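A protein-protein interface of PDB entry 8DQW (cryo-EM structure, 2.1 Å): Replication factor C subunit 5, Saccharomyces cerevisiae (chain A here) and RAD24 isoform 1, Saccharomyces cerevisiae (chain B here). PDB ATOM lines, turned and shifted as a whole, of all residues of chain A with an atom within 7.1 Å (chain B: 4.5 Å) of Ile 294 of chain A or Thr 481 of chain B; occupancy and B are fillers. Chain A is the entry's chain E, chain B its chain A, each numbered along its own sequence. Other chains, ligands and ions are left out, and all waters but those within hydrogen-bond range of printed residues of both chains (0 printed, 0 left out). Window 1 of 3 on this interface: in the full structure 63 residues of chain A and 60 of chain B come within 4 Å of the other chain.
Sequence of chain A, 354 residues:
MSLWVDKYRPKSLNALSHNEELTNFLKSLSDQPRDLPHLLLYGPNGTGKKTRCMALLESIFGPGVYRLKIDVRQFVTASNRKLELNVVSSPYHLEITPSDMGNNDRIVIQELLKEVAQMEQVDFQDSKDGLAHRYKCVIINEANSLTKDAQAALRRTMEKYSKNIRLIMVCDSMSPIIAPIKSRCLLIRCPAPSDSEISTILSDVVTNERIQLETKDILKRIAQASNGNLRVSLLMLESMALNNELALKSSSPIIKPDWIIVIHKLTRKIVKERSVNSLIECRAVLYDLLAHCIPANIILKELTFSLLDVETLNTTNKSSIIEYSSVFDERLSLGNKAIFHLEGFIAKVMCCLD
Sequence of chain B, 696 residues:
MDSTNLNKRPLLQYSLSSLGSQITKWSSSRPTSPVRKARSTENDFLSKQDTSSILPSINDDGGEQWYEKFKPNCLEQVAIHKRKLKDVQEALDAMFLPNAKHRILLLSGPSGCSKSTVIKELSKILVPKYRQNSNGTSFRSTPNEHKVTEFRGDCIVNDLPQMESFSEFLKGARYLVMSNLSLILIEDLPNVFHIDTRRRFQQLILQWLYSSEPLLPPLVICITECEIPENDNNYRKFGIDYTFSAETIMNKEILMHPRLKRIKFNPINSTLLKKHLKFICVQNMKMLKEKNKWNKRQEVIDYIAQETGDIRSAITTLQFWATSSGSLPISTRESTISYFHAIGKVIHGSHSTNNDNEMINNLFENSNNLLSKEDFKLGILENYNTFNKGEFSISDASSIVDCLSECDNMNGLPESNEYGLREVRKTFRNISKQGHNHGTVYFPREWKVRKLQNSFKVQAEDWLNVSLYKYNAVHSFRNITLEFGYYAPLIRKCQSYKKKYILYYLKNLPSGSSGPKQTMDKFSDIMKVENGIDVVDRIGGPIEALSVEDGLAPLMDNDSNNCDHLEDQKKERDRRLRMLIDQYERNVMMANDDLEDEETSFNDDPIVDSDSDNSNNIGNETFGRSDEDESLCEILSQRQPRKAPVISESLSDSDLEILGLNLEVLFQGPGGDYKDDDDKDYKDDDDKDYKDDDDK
NE1 of Trp 259 of chain A is in hydrogen-bond range of O of Leu 482 of chain B, at 2.9 Å.
O of Asp 288 of chain A is in hydrogen-bond range of ND1 of His 292 of chain A (3.4 Å).
The backbone carbonyl oxygen (O) of Arg 478 of chain B lies within hydrogen-bond range of the side-chain hydroxyl (OG1) of Thr 481 of chain B (2.5 Å).
Among the printed residues, pairs that only touch across the chains: Ile 294 of chain A with Thr 481 of chain B (3.1 Å), Pro 295 of chain A with Arg 478 of chain B (3.3 Å), Ile 298 of chain A with Arg 478 of chain B (3.4 Å), Cys 293 of chain A with Phe 456 of chain B (3.6 Å), His 292 of chain A with Phe 456 of chain B (3.6 Å), Cys 293 of chain A with Thr 481 of chain B (3.7 Å) and Cys 293 of chain A with Phe 477 of chain B (3.97 Å).
Of chain B, only Thr 481 (3.1 Å) comes within 4 Å of Ile 294 of chain A.
Ile 299 of chain A touches none of the printed residues of chain B.
Of the printed residues of chain A, Phe 456 of chain B touches His 292 (3.6 Å) and Cys 293 (3.6 Å).
Of the printed residues of chain A, Phe 477 of chain B touches Cys 293 (3.97 Å).
Of chain A, only Cys 293 (3.7 Å) and Ile 294 (3.1 Å) come within 4 Å of Thr 481 of chain B.
The nearest residue of chain A that does not touch Thr 481 of chain B is His 292 of chain A (4.3 Å).
The nearest printed residue of chain A that does not touch Leu 482 of chain B is Pro 295 of chain A (4.1 Å).
Of the 17 printed residues of chain A, 6 touch a printed residue of chain B.
Hydrophobic or aromatic side chains of chain A that line the printed part of chain B: Trp 259, Ile 294, Pro 295 and Ile 298.
Printed residues of chain B that touch a printed residue of chain A: Phe 456, Phe 477, Arg 478, Thr 481 and Leu 482.
Among the printed residues, no Asp or Glu carboxylate lies within 4 Å of a Lys or Arg side-chain nitrogen of the other chain.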
ATOM      1  N   ASP A 258      27.083   8.645   3.388  1.00  0.00           N
ATOM      2  CA  ASP A 258      27.210   8.504   1.940  1.00  0.00           C
ATOM      3  C   ASP A 258      26.012   7.773   1.346  1.00  0.00           C
ATOM      4  O   ASP A 258      25.511   8.151   0.278  1.00  0.00           O
ATOM      5  CB  ASP A 258      28.513   7.780   1.588  1.00  0.00           C
ATOM      6  CG  ASP A 258      28.787   6.585   2.485  1.00  0.00           C
ATOM      7  OD1 ASP A 258      28.195   6.507   3.581  1.00  0.00           O
ATOM      8  OD2 ASP A 258      29.603   5.726   2.094  1.00  0.00           O
ATOM      9  N   TRP A 259      25.540   6.721   2.018  1.00  0.00           N
ATOM     10  CA  TRP A 259      24.400   5.974   1.494  1.00  0.00           C
ATOM     11  C   TRP A 259      23.146   6.840   1.428  1.00  0.00           C
ATOM     12  O   TRP A 259      22.301   6.639   0.549  1.00  0.00           O
ATOM     13  CB  TRP A 259      24.155   4.721   2.339  1.00  0.00           C
ATOM     14  CG  TRP A 259      23.890   4.981   3.792  1.00  0.00           C
ATOM     15  CD1 TRP A 259      24.810   5.275   4.757  1.00  0.00           C
ATOM     16  CD2 TRP A 259      22.617   4.956   4.445  1.00  0.00           C
ATOM     17  NE1 TRP A 259      24.186   5.440   5.970  1.00  0.00           N
ATOM     18  CE2 TRP A 259      22.839   5.250   5.804  1.00  0.00           C
ATOM     19  CE3 TRP A 259      21.311   4.717   4.012  1.00  0.00           C
ATOM     20  CZ2 TRP A 259      21.803   5.310   6.733  1.00  0.00           C
ATOM     21  CZ3 TRP A 259      20.287   4.777   4.934  1.00  0.00           C
ATOM     22  CH2 TRP A 259      20.537   5.071   6.278  1.00  0.00           C
ATOM     23  N   ILE A 263      20.959   7.394  -1.903  1.00  0.00           N
ATOM     24  CA  ILE A 263      19.513   7.208  -1.992  1.00  0.00           C
ATOM     25  C   ILE A 263      18.848   8.458  -2.556  1.00  0.00           C
ATOM     26  O   ILE A 263      17.867   8.369  -3.302  1.00  0.00           O
ATOM     27  CB  ILE A 263      18.936   6.827  -0.617  1.00  0.00           C
ATOM     28  CG1 ILE A 263      19.208   5.349  -0.325  1.00  0.00           C
ATOM     29  CG2 ILE A 263      17.438   7.108  -0.565  1.00  0.00           C
ATOM     30  CD1 ILE A 263      18.994   4.961   1.119  1.00  0.00           C
ATOM     31  N   LEU A 286      20.560  -0.507  -5.843  1.00  0.00           N
ATOM     32  CA  LEU A 286      20.057  -1.205  -4.664  1.00  0.00           C
ATOM     33  C   LEU A 286      21.006  -2.313  -4.234  1.00  0.00           C
ATOM     34  O   LEU A 286      21.241  -2.513  -3.038  1.00  0.00           O
ATOM     35  CB  LEU A 286      18.669  -1.784  -4.944  1.00  0.00           C
ATOM     36  CG  LEU A 286      17.504  -0.806  -5.103  1.00  0.00           C
ATOM     37  CD1 LEU A 286      16.260  -1.557  -5.553  1.00  0.00           C
ATOM     38  CD2 LEU A 286      17.241  -0.046  -3.812  1.00  0.00           C
ATOM     39  N   ASP A 288      24.227  -2.397  -4.801  1.00  0.00           N
ATOM     40  CA  ASP A 288      25.386  -1.740  -4.203  1.00  0.00           C
ATOM     41  C   ASP A 288      25.105  -1.354  -2.756  1.00  0.00           C
ATOM     42  O   ASP A 288      25.958  -1.532  -1.879  1.00  0.00           O
ATOM     43  CB  ASP A 288      25.777  -0.510  -5.020  1.00  0.00           C
ATOM     44  CG  ASP A 288      27.062   0.129  -4.529  1.00  0.00           C
ATOM     45  OD1 ASP A 288      27.149   1.375  -4.533  1.00  0.00           O
ATOM     46  OD2 ASP A 288      27.986  -0.614  -4.138  1.00  0.00           O
ATOM     47  N   LEU A 289      23.910  -0.823  -2.486  1.00  0.00           N
ATOM     48  CA  LEU A 289      23.554  -0.471  -1.114  1.00  0.00           C
ATOM     49  C   LEU A 289      23.516  -1.704  -0.220  1.00  0.00           C
ATOM     50  O   LEU A 289      24.010  -1.677   0.914  1.00  0.00           O
ATOM     51  CB  LEU A 289      22.206   0.249  -1.087  1.00  0.00           C
ATOM     52  CG  LEU A 289      22.212   1.701  -1.571  1.00  0.00           C
ATOM     53  CD1 LEU A 289      20.791   2.192  -1.800  1.00  0.00           C
ATOM     54  CD2 LEU A 289      22.943   2.599  -0.583  1.00  0.00           C
ATOM     55  N   LEU A 290      22.932  -2.799  -0.714  1.00  0.00           N
ATOM     56  CA  LEU A 290      22.836  -4.017   0.085  1.00  0.00           C
ATOM     57  C   LEU A 290      24.206  -4.632   0.341  1.00  0.00           C
ATOM     58  O   LEU A 290      24.408  -5.284   1.372  1.00  0.00           O
ATOM     59  CB  LEU A 290      21.930  -5.033  -0.609  1.00  0.00           C
ATOM     60  CG  LEU A 290      20.428  -4.749  -0.565  1.00  0.00           C
ATOM     61  CD1 LEU A 290      19.695  -5.642  -1.553  1.00  0.00           C
ATOM     62  CD2 LEU A 290      19.877  -4.936   0.844  1.00  0.00           C
ATOM     63  N   ALA A 291      25.151  -4.447  -0.583  1.00  0.00           N
ATOM     64  CA  ALA A 291      26.490  -4.994  -0.398  1.00  0.00           C
ATOM     65  C   ALA A 291      27.186  -4.412   0.824  1.00  0.00           C
ATOM     66  O   ALA A 291      28.103  -5.043   1.360  1.00  0.00           O
ATOM     67  CB  ALA A 291      27.335  -4.740  -1.646  1.00  0.00           C
ATOM     68  N   HIS A 292      26.777  -3.228   1.271  1.00  0.00           N
ATOM     69  CA  HIS A 292      27.327  -2.605   2.466  1.00  0.00           C
ATOM     70  C   HIS A 292      26.541  -2.962   3.723  1.00  0.00           C
ATOM     71  O   HIS A 292      26.717  -2.312   4.758  1.00  0.00           O
ATOM     72  CB  HIS A 292      27.375  -1.084   2.290  1.00  0.00           C
ATOM     73  CG  HIS A 292      28.541  -0.607   1.482  1.00  0.00           C
ATOM     74  ND1 HIS A 292      28.599  -0.734   0.110  1.00  0.00           N
ATOM     75  CD2 HIS A 292      29.697  -0.007   1.852  1.00  0.00           C
ATOM     76  CE1 HIS A 292      29.738  -0.230  -0.330  1.00  0.00           C
ATOM     77  NE2 HIS A 292      30.422   0.218   0.707  1.00  0.00           N
ATOM     78  N   CYS A 293      25.676  -3.975   3.649  1.00  0.00           N
ATOM     79  CA  CYS A 293      24.932  -4.475   4.805  1.00  0.00           C
ATOM     80  C   CYS A 293      23.956  -3.439   5.352  1.00  0.00           C
ATOM     81  O   CYS A 293      23.615  -3.459   6.537  1.00  0.00           O
ATOM     82  CB  CYS A 293      25.882  -4.946   5.909  1.00  0.00           C
ATOM     83  SG  CYS A 293      27.149  -6.104   5.344  1.00  0.00           S
ATOM     84  N   ILE A 294      23.496  -2.527   4.505  1.00  0.00           N
ATOM     85  CA  ILE A 294      22.414  -1.626   4.915  1.00  0.00           C
ATOM     86  C   ILE A 294      21.108  -2.416   4.961  1.00  0.00           C
ATOM     87  O   ILE A 294      20.755  -3.071   3.965  1.00  0.00           O
ATOM     88  CB  ILE A 294      22.307  -0.443   3.949  1.00  0.00           C
ATOM     89  CG1 ILE A 294      23.643   0.302   3.845  1.00  0.00           C
ATOM     90  CG2 ILE A 294      21.204   0.510   4.397  1.00  0.00           C
ATOM     91  CD1 ILE A 294      24.174   0.836   5.163  1.00  0.00           C
ATOM     92  N   PRO A 295      20.369  -2.404   6.071  1.00  0.00           N
ATOM     93  CA  PRO A 295      19.137  -3.204   6.134  1.00  0.00           C
ATOM     94  C   PRO A 295      18.147  -2.800   5.049  1.00  0.00           C
ATOM     95  O   PRO A 295      18.030  -1.627   4.691  1.00  0.00           O
ATOM     96  CB  PRO A 295      18.586  -2.911   7.535  1.00  0.00           C
ATOM     97  CG  PRO A 295      19.725  -2.375   8.316  1.00  0.00           C
ATOM     98  CD  PRO A 295      20.676  -1.744   7.353  1.00  0.00           C
ATOM     99  N   ALA A 296      17.424  -3.796   4.530  1.00  0.00           N
ATOM    100  CA  ALA A 296      16.473  -3.542   3.451  1.00  0.00           C
ATOM    101  C   ALA A 296      15.357  -2.603   3.895  1.00  0.00           C
ATOM    102  O   ALA A 296      14.966  -1.695   3.149  1.00  0.00           O
ATOM    103  CB  ALA A 296      15.891  -4.863   2.949  1.00  0.00           C
ATOM    104  N   ASN A 297      14.826  -2.803   5.104  1.00  0.00           N
ATOM    105  CA  ASN A 297      13.733  -1.958   5.575  1.00  0.00           C
ATOM    106  C   ASN A 297      14.186  -0.511   5.734  1.00  0.00           C
ATOM    107  O   ASN A 297      13.418   0.424   5.469  1.00  0.00           O
ATOM    108  CB  ASN A 297      13.179  -2.500   6.895  1.00  0.00           C
ATOM    109  CG  ASN A 297      14.180  -2.412   8.030  1.00  0.00           C
ATOM    110  OD1 ASN A 297      15.222  -3.066   8.006  1.00  0.00           O
ATOM    111  ND2 ASN A 297      13.871  -1.595   9.030  1.00  0.00           N
ATOM    112  N   ILE A 298      15.429  -0.305   6.173  1.00  0.00           N
ATOM    113  CA  ILE A 298      15.967   1.049   6.275  1.00  0.00           C
ATOM    114  C   ILE A 298      16.047   1.690   4.896  1.00  0.00           C
ATOM    115  O   ILE A 298      15.699   2.864   4.715  1.00  0.00           O
ATOM    116  CB  ILE A 298      17.341   1.027   6.970  1.00  0.00           C
ATOM    117  CG1 ILE A 298      17.192   0.600   8.433  1.00  0.00           C
ATOM    118  CG2 ILE A 298      18.017   2.387   6.863  1.00  0.00           C
ATOM    119  CD1 ILE A 298      16.584   1.662   9.326  1.00  0.00           C
ATOM    120  N   ILE A 299      16.515   0.931   3.903  1.00  0.00           N
ATOM    121  CA  ILE A 299      16.553   1.446   2.539  1.00  0.00           C
ATOM    122  C   ILE A 299      15.154   1.843   2.093  1.00  0.00           C
ATOM    123  O   ILE A 299      14.963   2.887   1.458  1.00  0.00           O
ATOM    124  CB  ILE A 299      17.181   0.410   1.588  1.00  0.00           C
ATOM    125  CG1 ILE A 299      18.636   0.142   1.982  1.00  0.00           C
ATOM    126  CG2 ILE A 299      17.112   0.898   0.144  1.00  0.00           C
ATOM    127  CD1 ILE A 299      19.244  -1.085   1.331  1.00  0.00           C
ATOM    128  N   GLU A 302      14.079   5.141   3.778  1.00  0.00           N
ATOM    129  CA  GLU A 302      14.783   6.326   3.308  1.00  0.00           C
ATOM    130  C   GLU A 302      14.366   6.673   1.886  1.00  0.00           C
ATOM    131  O   GLU A 302      14.132   7.844   1.569  1.00  0.00           O
ATOM    132  CB  GLU A 302      16.292   6.117   3.414  1.00  0.00           C
ATOM    133  CG  GLU A 302      16.763   5.830   4.830  1.00  0.00           C
ATOM    134  CD  GLU A 302      16.522   6.992   5.769  1.00  0.00           C
ATOM    135  OE1 GLU A 302      17.375   7.902   5.828  1.00  0.00           O
ATOM    136  OE2 GLU A 302      15.474   6.996   6.449  1.00  0.00           O
ATOM    137  N   PHE B 456      32.548  -7.194   4.340  1.00  0.00           N
ATOM    138  CA  PHE B 456      32.152  -6.079   5.192  1.00  0.00           C
ATOM    139  C   PHE B 456      32.053  -6.517   6.645  1.00  0.00           C
ATOM    140  O   PHE B 456      32.443  -5.774   7.550  1.00  0.00           O
ATOM    141  CB  PHE B 456      30.818  -5.500   4.719  1.00  0.00           C
ATOM    142  CG  PHE B 456      30.417  -4.238   5.434  1.00  0.00           C
ATOM    143  CD1 PHE B 456      29.891  -4.284   6.715  1.00  0.00           C
ATOM    144  CD2 PHE B 456      30.565  -3.006   4.822  1.00  0.00           C
ATOM    145  CE1 PHE B 456      29.527  -3.125   7.373  1.00  0.00           C
ATOM    146  CE2 PHE B 456      30.201  -1.845   5.473  1.00  0.00           C
ATOM    147  CZ  PHE B 456      29.679  -1.905   6.750  1.00  0.00           C
ATOM    148  N   PHE B 477      26.899  -3.530  15.602  1.00  0.00           N
ATOM    149  CA  PHE B 477      27.159  -3.701  14.176  1.00  0.00           C
ATOM    150  C   PHE B 477      26.208  -2.854  13.340  1.00  0.00           C
ATOM    151  O   PHE B 477      26.599  -2.310  12.300  1.00  0.00           O
ATOM    152  CB  PHE B 477      27.037  -5.178  13.801  1.00  0.00           C
ATOM    153  CG  PHE B 477      27.042  -5.429  12.322  1.00  0.00           C
ATOM    154  CD1 PHE B 477      28.236  -5.552  11.633  1.00  0.00           C
ATOM    155  CD2 PHE B 477      25.853  -5.545  11.621  1.00  0.00           C
ATOM    156  CE1 PHE B 477      28.244  -5.783  10.271  1.00  0.00           C
ATOM    157  CE2 PHE B 477      25.856  -5.776  10.260  1.00  0.00           C
ATOM    158  CZ  PHE B 477      27.053  -5.894   9.585  1.00  0.00           C
ATOM    159  N   ARG B 478      24.952  -2.737  13.775  1.00  0.00           N
ATOM    160  CA  ARG B 478      23.979  -1.935  13.039  1.00  0.00           C
ATOM    161  C   ARG B 478      24.446  -0.489  12.918  1.00  0.00           C
ATOM    162  O   ARG B 478      24.403   0.104  11.833  1.00  0.00           O
ATOM    163  CB  ARG B 478      22.620  -2.006  13.738  1.00  0.00           C
ATOM    164  CG  ARG B 478      21.481  -1.344  12.979  1.00  0.00           C
ATOM    165  CD  ARG B 478      20.145  -1.609  13.660  1.00  0.00           C
ATOM    166  NE  ARG B 478      19.011  -1.187  12.847  1.00  0.00           N
ATOM    167  CZ  ARG B 478      18.493  -1.894  11.852  1.00  0.00           C
ATOM    168  NH1 ARG B 478      18.989  -3.071  11.507  1.00  0.00           N
ATOM    169  NH2 ARG B 478      17.451  -1.406  11.184  1.00  0.00           N
ATOM    170  N   ASN B 479      24.903   0.095  14.029  1.00  0.00           N
ATOM    171  CA  ASN B 479      25.386   1.471  13.989  1.00  0.00           C
ATOM    172  C   ASN B 479      26.629   1.598  13.120  1.00  0.00           C
ATOM    173  O   ASN B 479      26.856   2.652  12.514  1.00  0.00           O
ATOM    174  CB  ASN B 479      25.672   1.966  15.407  1.00  0.00           C
ATOM    175  CG  ASN B 479      24.403   2.276  16.181  1.00  0.00           C
ATOM    176  OD1 ASN B 479      23.350   2.526  15.594  1.00  0.00           O
ATOM    177  ND2 ASN B 479      24.498   2.259  17.504  1.00  0.00           N
ATOM    178  N   ILE B 480      27.446   0.546  13.050  1.00  0.00           N
ATOM    179  CA  ILE B 480      28.600   0.569  12.158  1.00  0.00           C
ATOM    180  C   ILE B 480      28.145   0.603  10.705  1.00  0.00           C
ATOM    181  O   ILE B 480      28.683   1.362   9.890  1.00  0.00           O
ATOM    182  CB  ILE B 480      29.519  -0.633  12.440  1.00  0.00           C
ATOM    183  CG1 ILE B 480      30.243  -0.440  13.774  1.00  0.00           C
ATOM    184  CG2 ILE B 480      30.527  -0.807  11.313  1.00  0.00           C
ATOM    185  CD1 ILE B 480      30.792  -1.719  14.363  1.00  0.00           C
ATOM    186  N   THR B 481      27.145  -0.210  10.355  1.00  0.00           N
ATOM    187  CA  THR B 481      26.642  -0.200   8.984  1.00  0.00           C
ATOM    188  C   THR B 481      26.006   1.141   8.644  1.00  0.00           C
ATOM    189  O   THR B 481      26.117   1.618   7.509  1.00  0.00           O
ATOM    190  CB  THR B 481      25.631  -1.329   8.772  1.00  0.00           C
ATOM    191  OG1 THR B 481      24.512  -1.149   9.648  1.00  0.00           O
ATOM    192  CG2 THR B 481      26.270  -2.685   9.031  1.00  0.00           C
ATOM    193  N   LEU B 482      25.335   1.763   9.611  1.00  0.00           N
ATOM    194  CA  LEU B 482      24.600   2.992   9.341  1.00  0.00           C
ATOM    195  C   LEU B 482      25.473   4.239   9.462  1.00  0.00           C
ATOM    196  O   LEU B 482      25.505   5.059   8.540  1.00  0.00           O
ATOM    197  CB  LEU B 482      23.397   3.099  10.283  1.00  0.00           C
ATOM    198  CG  LEU B 482      22.327   2.011  10.139  1.00  0.00           C
ATOM    199  CD1 LEU B 482      21.195   2.244  11.124  1.00  0.00           C
ATOM    200  CD2 LEU B 482      21.789   1.947   8.715  1.00  0.00           C
ATOM    201  N   GLU B 483      26.178   4.405  10.582  1.00  0.00           N
ATOM    202  CA  GLU B 483      26.863   5.663  10.869  1.00  0.00           C
ATOM    203  C   GLU B 483      28.379   5.519  10.947  1.00  0.00           C
ATOM    204  O   GLU B 483      29.091   6.179  10.184  1.00  0.00           O
ATOM    205  CB  GLU B 483      26.317   6.253  12.176  1.00  0.00           C
ATOM    206  CG  GLU B 483      24.806   6.434  12.195  1.00  0.00           C
ATOM    207  CD  GLU B 483      24.231   6.424  13.598  1.00  0.00           C
ATOM    208  OE1 GLU B 483      24.898   6.941  14.519  1.00  0.00           O
ATOM    209  OE2 GLU B 483      23.114   5.899  13.780  1.00  0.00           O
